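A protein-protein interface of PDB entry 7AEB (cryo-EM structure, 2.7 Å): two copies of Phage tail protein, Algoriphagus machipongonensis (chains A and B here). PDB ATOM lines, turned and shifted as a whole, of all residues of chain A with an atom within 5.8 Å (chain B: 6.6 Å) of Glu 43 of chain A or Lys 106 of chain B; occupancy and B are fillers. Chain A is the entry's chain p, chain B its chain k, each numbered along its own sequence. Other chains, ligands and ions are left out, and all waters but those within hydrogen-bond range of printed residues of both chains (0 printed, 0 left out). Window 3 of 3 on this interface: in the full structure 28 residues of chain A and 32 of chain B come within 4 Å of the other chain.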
ATOM      1  N   ARG A  37      19.207  10.881   0.029  1.00  0.00           N
ATOM      2  CA  ARG A  37      19.185  12.137  -0.740  1.00  0.00           C
ATOM      3  C   ARG A  37      18.261  12.082  -1.959  1.00  0.00           C
ATOM      4  O   ARG A  37      18.393  11.199  -2.802  1.00  0.00           O
ATOM      5  CB  ARG A  37      20.573  12.567  -1.235  1.00  0.00           C
ATOM      6  CG  ARG A  37      20.543  13.869  -2.065  1.00  0.00           C
ATOM      7  CD  ARG A  37      21.855  14.410  -2.529  1.00  0.00           C
ATOM      8  NE  ARG A  37      21.614  15.648  -3.316  1.00  0.00           N
ATOM      9  CZ  ARG A  37      21.349  15.693  -4.664  1.00  0.00           C
ATOM     10  NH1 ARG A  37      21.368  14.586  -5.380  1.00  0.00           N
ATOM     11  NH2 ARG A  37      21.054  16.835  -5.280  1.00  0.00           N
ATOM     12  N   SER A  41      17.385  18.053  -4.279  1.00  0.00           N
ATOM     13  CA  SER A  41      17.908  18.835  -3.165  1.00  0.00           C
ATOM     14  C   SER A  41      19.041  19.804  -3.562  1.00  0.00           C
ATOM     15  O   SER A  41      19.953  19.416  -4.291  1.00  0.00           O
ATOM     16  CB  SER A  41      18.439  17.929  -2.085  1.00  0.00           C
ATOM     17  OG  SER A  41      19.033  18.688  -1.056  1.00  0.00           O
ATOM     18  N   PRO A  42      19.030  21.076  -3.084  1.00  0.00           N
ATOM     19  CA  PRO A  42      20.087  22.077  -3.222  1.00  0.00           C
ATOM     20  C   PRO A  42      21.419  21.678  -2.577  1.00  0.00           C
ATOM     21  O   PRO A  42      22.449  22.279  -2.862  1.00  0.00           O
ATOM     22  CB  PRO A  42      19.506  23.287  -2.491  1.00  0.00           C
ATOM     23  CG  PRO A  42      18.044  23.101  -2.537  1.00  0.00           C
ATOM     24  CD  PRO A  42      17.815  21.619  -2.468  1.00  0.00           C
ATOM     25  N   GLU A  43      21.392  20.725  -1.642  1.00  0.00           N
ATOM     26  CA  GLU A  43      22.627  20.293  -1.009  1.00  0.00           C
ATOM     27  C   GLU A  43      23.077  19.018  -1.663  1.00  0.00           C
ATOM     28  O   GLU A  43      22.259  18.165  -2.008  1.00  0.00           O
ATOM     29  CB  GLU A  43      22.481  20.100   0.498  1.00  0.00           C
ATOM     30  CG  GLU A  43      22.238  21.366   1.265  1.00  0.00           C
ATOM     31  CD  GLU A  43      22.198  21.150   2.760  1.00  0.00           C
ATOM     32  OE1 GLU A  43      22.122  20.022   3.169  1.00  0.00           O
ATOM     33  OE2 GLU A  43      22.257  22.110   3.484  1.00  0.00           O
ATOM     34  N   TYR A  44      24.381  18.838  -1.750  1.00  0.00           N
ATOM     35  CA  TYR A  44      24.944  17.690  -2.424  1.00  0.00           C
ATOM     36  C   TYR A  44      25.535  16.668  -1.467  1.00  0.00           C
ATOM     37  O   TYR A  44      26.560  16.053  -1.741  1.00  0.00           O
ATOM     38  CB  TYR A  44      25.935  18.183  -3.463  1.00  0.00           C
ATOM     39  CG  TYR A  44      25.279  19.230  -4.372  1.00  0.00           C
ATOM     40  CD1 TYR A  44      25.799  20.497  -4.437  1.00  0.00           C
ATOM     41  CD2 TYR A  44      24.118  18.941  -5.068  1.00  0.00           C
ATOM     42  CE1 TYR A  44      25.196  21.459  -5.200  1.00  0.00           C
ATOM     43  CE2 TYR A  44      23.509  19.908  -5.822  1.00  0.00           C
ATOM     44  CZ  TYR A  44      24.049  21.164  -5.889  1.00  0.00           C
ATOM     45  OH  TYR A  44      23.449  22.137  -6.644  1.00  0.00           O
ATOM     46  N   SER A  45      24.866  16.508  -0.338  1.00  0.00           N
ATOM     47  CA  SER A  45      25.221  15.579   0.712  1.00  0.00           C
ATOM     48  C   SER A  45      23.942  14.931   1.234  1.00  0.00           C
ATOM     49  O   SER A  45      22.839  15.327   0.855  1.00  0.00           O
ATOM     50  CB  SER A  45      25.974  16.290   1.811  1.00  0.00           C
ATOM     51  OG  SER A  45      25.157  17.219   2.447  1.00  0.00           O
ATOM     52  N   MET B  52      30.184  15.013  -5.546  1.00  0.00           N
ATOM     53  CA  MET B  52      29.395  15.140  -4.318  1.00  0.00           C
ATOM     54  C   MET B  52      30.288  15.306  -3.082  1.00  0.00           C
ATOM     55  O   MET B  52      31.474  14.958  -3.110  1.00  0.00           O
ATOM     56  CB  MET B  52      28.466  13.952  -4.167  1.00  0.00           C
ATOM     57  CG  MET B  52      27.377  13.908  -5.231  1.00  0.00           C
ATOM     58  SD  MET B  52      26.260  12.510  -5.092  1.00  0.00           S
ATOM     59  CE  MET B  52      25.269  12.962  -3.676  1.00  0.00           C
ATOM     60  N   ARG B  86      21.104  18.189  17.952  1.00  0.00           N
ATOM     61  CA  ARG B  86      21.601  19.441  18.522  1.00  0.00           C
ATOM     62  C   ARG B  86      22.595  20.216  17.658  1.00  0.00           C
ATOM     63  O   ARG B  86      23.323  19.665  16.828  1.00  0.00           O
ATOM     64  CB  ARG B  86      22.277  19.163  19.861  1.00  0.00           C
ATOM     65  CG  ARG B  86      21.392  18.531  20.936  1.00  0.00           C
ATOM     66  CD  ARG B  86      22.108  18.352  22.218  1.00  0.00           C
ATOM     67  NE  ARG B  86      21.311  17.617  23.166  1.00  0.00           N
ATOM     68  CZ  ARG B  86      21.712  17.192  24.375  1.00  0.00           C
ATOM     69  NH1 ARG B  86      22.930  17.452  24.822  1.00  0.00           N
ATOM     70  NH2 ARG B  86      20.859  16.504  25.121  1.00  0.00           N
ATOM     71  N   ASP B  87      22.661  21.511  17.911  1.00  0.00           N
ATOM     72  CA  ASP B  87      23.658  22.375  17.295  1.00  0.00           C
ATOM     73  C   ASP B  87      24.912  22.371  18.147  1.00  0.00           C
ATOM     74  O   ASP B  87      24.854  22.633  19.348  1.00  0.00           O
ATOM     75  CB  ASP B  87      23.129  23.782  17.110  1.00  0.00           C
ATOM     76  CG  ASP B  87      22.051  23.863  16.032  1.00  0.00           C
ATOM     77  OD1 ASP B  87      22.003  23.021  15.154  1.00  0.00           O
ATOM     78  OD2 ASP B  87      21.271  24.769  16.105  1.00  0.00           O
ATOM     79  N   LEU B  88      26.018  21.978  17.546  1.00  0.00           N
ATOM     80  CA  LEU B  88      27.300  21.848  18.221  1.00  0.00           C
ATOM     81  C   LEU B  88      28.257  22.993  17.886  1.00  0.00           C
ATOM     82  O   LEU B  88      28.574  23.229  16.718  1.00  0.00           O
ATOM     83  CB  LEU B  88      27.882  20.474  17.833  1.00  0.00           C
ATOM     84  CG  LEU B  88      29.322  20.095  18.265  1.00  0.00           C
ATOM     85  CD1 LEU B  88      29.416  19.960  19.766  1.00  0.00           C
ATOM     86  CD2 LEU B  88      29.714  18.798  17.564  1.00  0.00           C
ATOM     87  N   LYS B 104      31.246  25.526  13.353  1.00  0.00           N
ATOM     88  CA  LYS B 104      29.804  25.400  13.541  1.00  0.00           C
ATOM     89  C   LYS B 104      29.244  24.130  12.917  1.00  0.00           C
ATOM     90  O   LYS B 104      29.341  23.936  11.704  1.00  0.00           O
ATOM     91  CB  LYS B 104      29.129  26.618  12.941  1.00  0.00           C
ATOM     92  CG  LYS B 104      29.497  27.898  13.629  1.00  0.00           C
ATOM     93  CD  LYS B 104      28.838  29.075  12.991  1.00  0.00           C
ATOM     94  CE  LYS B 104      29.190  30.346  13.708  1.00  0.00           C
ATOM     95  NZ  LYS B 104      28.543  31.523  13.085  1.00  0.00           N
ATOM     96  N   VAL B 105      28.644  23.260  13.738  1.00  0.00           N
ATOM     97  CA  VAL B 105      28.132  21.975  13.272  1.00  0.00           C
ATOM     98  C   VAL B 105      26.610  21.811  13.403  1.00  0.00           C
ATOM     99  O   VAL B 105      26.016  21.952  14.478  1.00  0.00           O
ATOM    100  CB  VAL B 105      28.879  20.851  14.013  1.00  0.00           C
ATOM    101  CG1 VAL B 105      28.337  19.497  13.622  1.00  0.00           C
ATOM    102  CG2 VAL B 105      30.338  20.923  13.678  1.00  0.00           C
ATOM    103  N   LYS B 106      25.993  21.482  12.275  1.00  0.00           N
ATOM    104  CA  LYS B 106      24.545  21.298  12.106  1.00  0.00           C
ATOM    105  C   LYS B 106      24.011  19.868  12.377  1.00  0.00           C
ATOM    106  O   LYS B 106      24.539  18.895  11.836  1.00  0.00           O
ATOM    107  CB  LYS B 106      24.231  21.703  10.665  1.00  0.00           C
ATOM    108  CG  LYS B 106      22.792  21.686  10.246  1.00  0.00           C
ATOM    109  CD  LYS B 106      22.610  22.308   8.846  1.00  0.00           C
ATOM    110  CE  LYS B 106      23.209  21.411   7.742  1.00  0.00           C
ATOM    111  NZ  LYS B 106      22.900  21.896   6.391  1.00  0.00           N
ATOM    112  N   ASN B 107      22.912  19.757  13.119  1.00  0.00           N
ATOM    113  CA  ASN B 107      22.194  18.491  13.343  1.00  0.00           C
ATOM    114  C   ASN B 107      22.911  17.269  13.924  1.00  0.00           C
ATOM    115  O   ASN B 107      22.668  16.166  13.480  1.00  0.00           O
ATOM    116  CB  ASN B 107      21.553  18.043  12.015  1.00  0.00           C
ATOM    117  CG  ASN B 107      20.335  18.856  11.624  1.00  0.00           C
ATOM    118  OD1 ASN B 107      19.800  19.609  12.409  1.00  0.00           O
ATOM    119  ND2 ASN B 107      19.903  18.700  10.398  1.00  0.00           N
ATOM    120  N   ALA B 108      23.789  17.432  14.891  1.00  0.00           N
ATOM    121  CA  ALA B 108      24.500  16.286  15.435  1.00  0.00           C
ATOM    122  C   ALA B 108      23.703  15.366  16.371  1.00  0.00           C
ATOM    123  O   ALA B 108      22.808  15.809  17.055  1.00  0.00           O
ATOM    124  CB  ALA B 108      25.792  16.743  16.091  1.00  0.00           C
ATOM    125  N   ALA B 133      27.490  11.943  14.588  1.00  0.00           N
ATOM    126  CA  ALA B 133      27.111  12.115  13.193  1.00  0.00           C
ATOM    127  C   ALA B 133      26.600  13.536  13.027  1.00  0.00           C
ATOM    128  O   ALA B 133      26.062  14.100  13.976  1.00  0.00           O
ATOM    129  CB  ALA B 133      26.044  11.119  12.793  1.00  0.00           C
ATOM    130  N   HIS B 134      26.743  14.129  11.849  1.00  0.00           N
ATOM    131  CA  HIS B 134      26.206  15.477  11.631  1.00  0.00           C
ATOM    132  C   HIS B 134      25.954  15.717  10.152  1.00  0.00           C
ATOM    133  O   HIS B 134      26.273  14.867   9.321  1.00  0.00           O
ATOM    134  CB  HIS B 134      27.141  16.530  12.216  1.00  0.00           C
ATOM    135  CG  HIS B 134      28.433  16.618  11.552  1.00  0.00           C
ATOM    136  ND1 HIS B 134      28.695  17.486  10.510  1.00  0.00           N
ATOM    137  CD2 HIS B 134      29.545  15.904  11.742  1.00  0.00           C
ATOM    138  CE1 HIS B 134      29.932  17.304  10.119  1.00  0.00           C
ATOM    139  NE2 HIS B 134      30.459  16.330  10.845  1.00  0.00           N
ATOM    140  N   GLU B 135      25.345  16.855   9.830  1.00  0.00           N
ATOM    141  CA  GLU B 135      25.013  17.203   8.448  1.00  0.00           C
ATOM    142  C   GLU B 135      25.703  18.444   7.869  1.00  0.00           C
ATOM    143  O   GLU B 135      25.195  19.029   6.911  1.00  0.00           O
ATOM    144  CB  GLU B 135      23.494  17.345   8.305  1.00  0.00           C
ATOM    145  CG  GLU B 135      22.723  16.041   8.539  1.00  0.00           C
ATOM    146  CD  GLU B 135      21.230  16.164   8.363  1.00  0.00           C
ATOM    147  OE1 GLU B 135      20.759  17.260   8.208  1.00  0.00           O
ATOM    148  OE2 GLU B 135      20.565  15.164   8.396  1.00  0.00           O
ATOM    149  N   GLY B 136      26.835  18.880   8.419  1.00  0.00           N
ATOM    150  CA  GLY B 136      27.481  20.043   7.831  1.00  0.00           C
ATOM    151  C   GLY B 136      28.309  20.871   8.787  1.00  0.00           C
ATOM    152  O   GLY B 136      27.963  21.061   9.956  1.00  0.00           O
ATOM    153  N   LEU B 137      29.389  21.425   8.240  1.00  0.00           N
ATOM    154  CA  LEU B 137      30.371  22.224   8.956  1.00  0.00           C
ATOM    155  C   LEU B 137      30.764  23.524   8.257  1.00  0.00           C
ATOM    156  O   LEU B 137      31.139  23.530   7.088  1.00  0.00           O
ATOM    157  CB  LEU B 137      31.630  21.355   9.195  1.00  0.00           C
ATOM    158  CG  LEU B 137      32.907  22.053   9.764  1.00  0.00           C
ATOM    159  CD1 LEU B 137      32.663  22.572  11.154  1.00  0.00           C
ATOM    160  CD2 LEU B 137      34.070  21.040   9.782  1.00  0.00           C
ATOM    161  N   VAL B 138      30.708  24.617   9.015  1.00  0.00           N
ATOM    162  CA  VAL B 138      31.120  25.952   8.579  1.00  0.00           C
ATOM    163  C   VAL B 138      32.244  26.489   9.471  1.00  0.00           C
ATOM    164  O   VAL B 138      32.180  26.388  10.698  1.00  0.00           O
ATOM    165  CB  VAL B 138      29.924  26.927   8.554  1.00  0.00           C
ATOM    166  CG1 VAL B 138      30.368  28.329   8.172  1.00  0.00           C
ATOM    167  CG2 VAL B 138      28.901  26.434   7.560  1.00  0.00           C
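NZ of Lys 106 of chain B is in salt-bridge range of OE2 of Glu 43 of chain A, at 3.0 Å.
N of Glu 135 of chain B is in hydrogen-bond range of O of Lys 106 of chain B. O of Gly 136 of chain B is in hydrogen-bond range of N of Lys 106 of chain B, at 3.1 Å. The guanidinium group (NH2) of Arg 37 of chain A is in hydrogen-bond range of the backbone carbonyl oxygen (O) of Ser 41 of chain A (3.0 Å). The guanidinium group (NE) of Arg 37 of chain A is in hydrogen-bond range of the backbone carbonyl oxygen (O) of Glu 43 of chain A (2.9 Å). The backbone NH (N) of Glu 43 of chain A lies within hydrogen-bond range of the side-chain hydroxyl (OG) of Ser 41 of chain A, at 3.2 Å.
Among the printed residues, pairs that only touch across the chains: Tyr 44 of chain A with Met 52 of chain B (3.7 Å) and Arg 37 of chain A with Met 52 of chain B (3.9 Å).
Of the printed residues of chain B, Arg 37 of chain A touches Met 52. Glu 43 of chain A touches just one residue of chain B: Lys 106. Printed residues of chain B within 4 Å of Tyr 44 of chain A: Met 52. Of the printed residues of chain A, Met 52 of chain B touches Arg 37 (3.9 Å) and Tyr 44 (3.7 Å). Lys 106 of chain B touches one residue of chain A.
Of the 6 printed residues of chain A, 3 touch a printed residue of chain B. Printed residues of chain A that touch a printed residue of chain B: Arg 37, Glu 43 and Tyr 44. Of the 15 printed residues of chain B, 2 touch a printed residue of chain A.
No position is printed for both chains. Of the 3 pairs that touch across the chains among the printed residues, none has its exchanged pair printed and touching as well.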
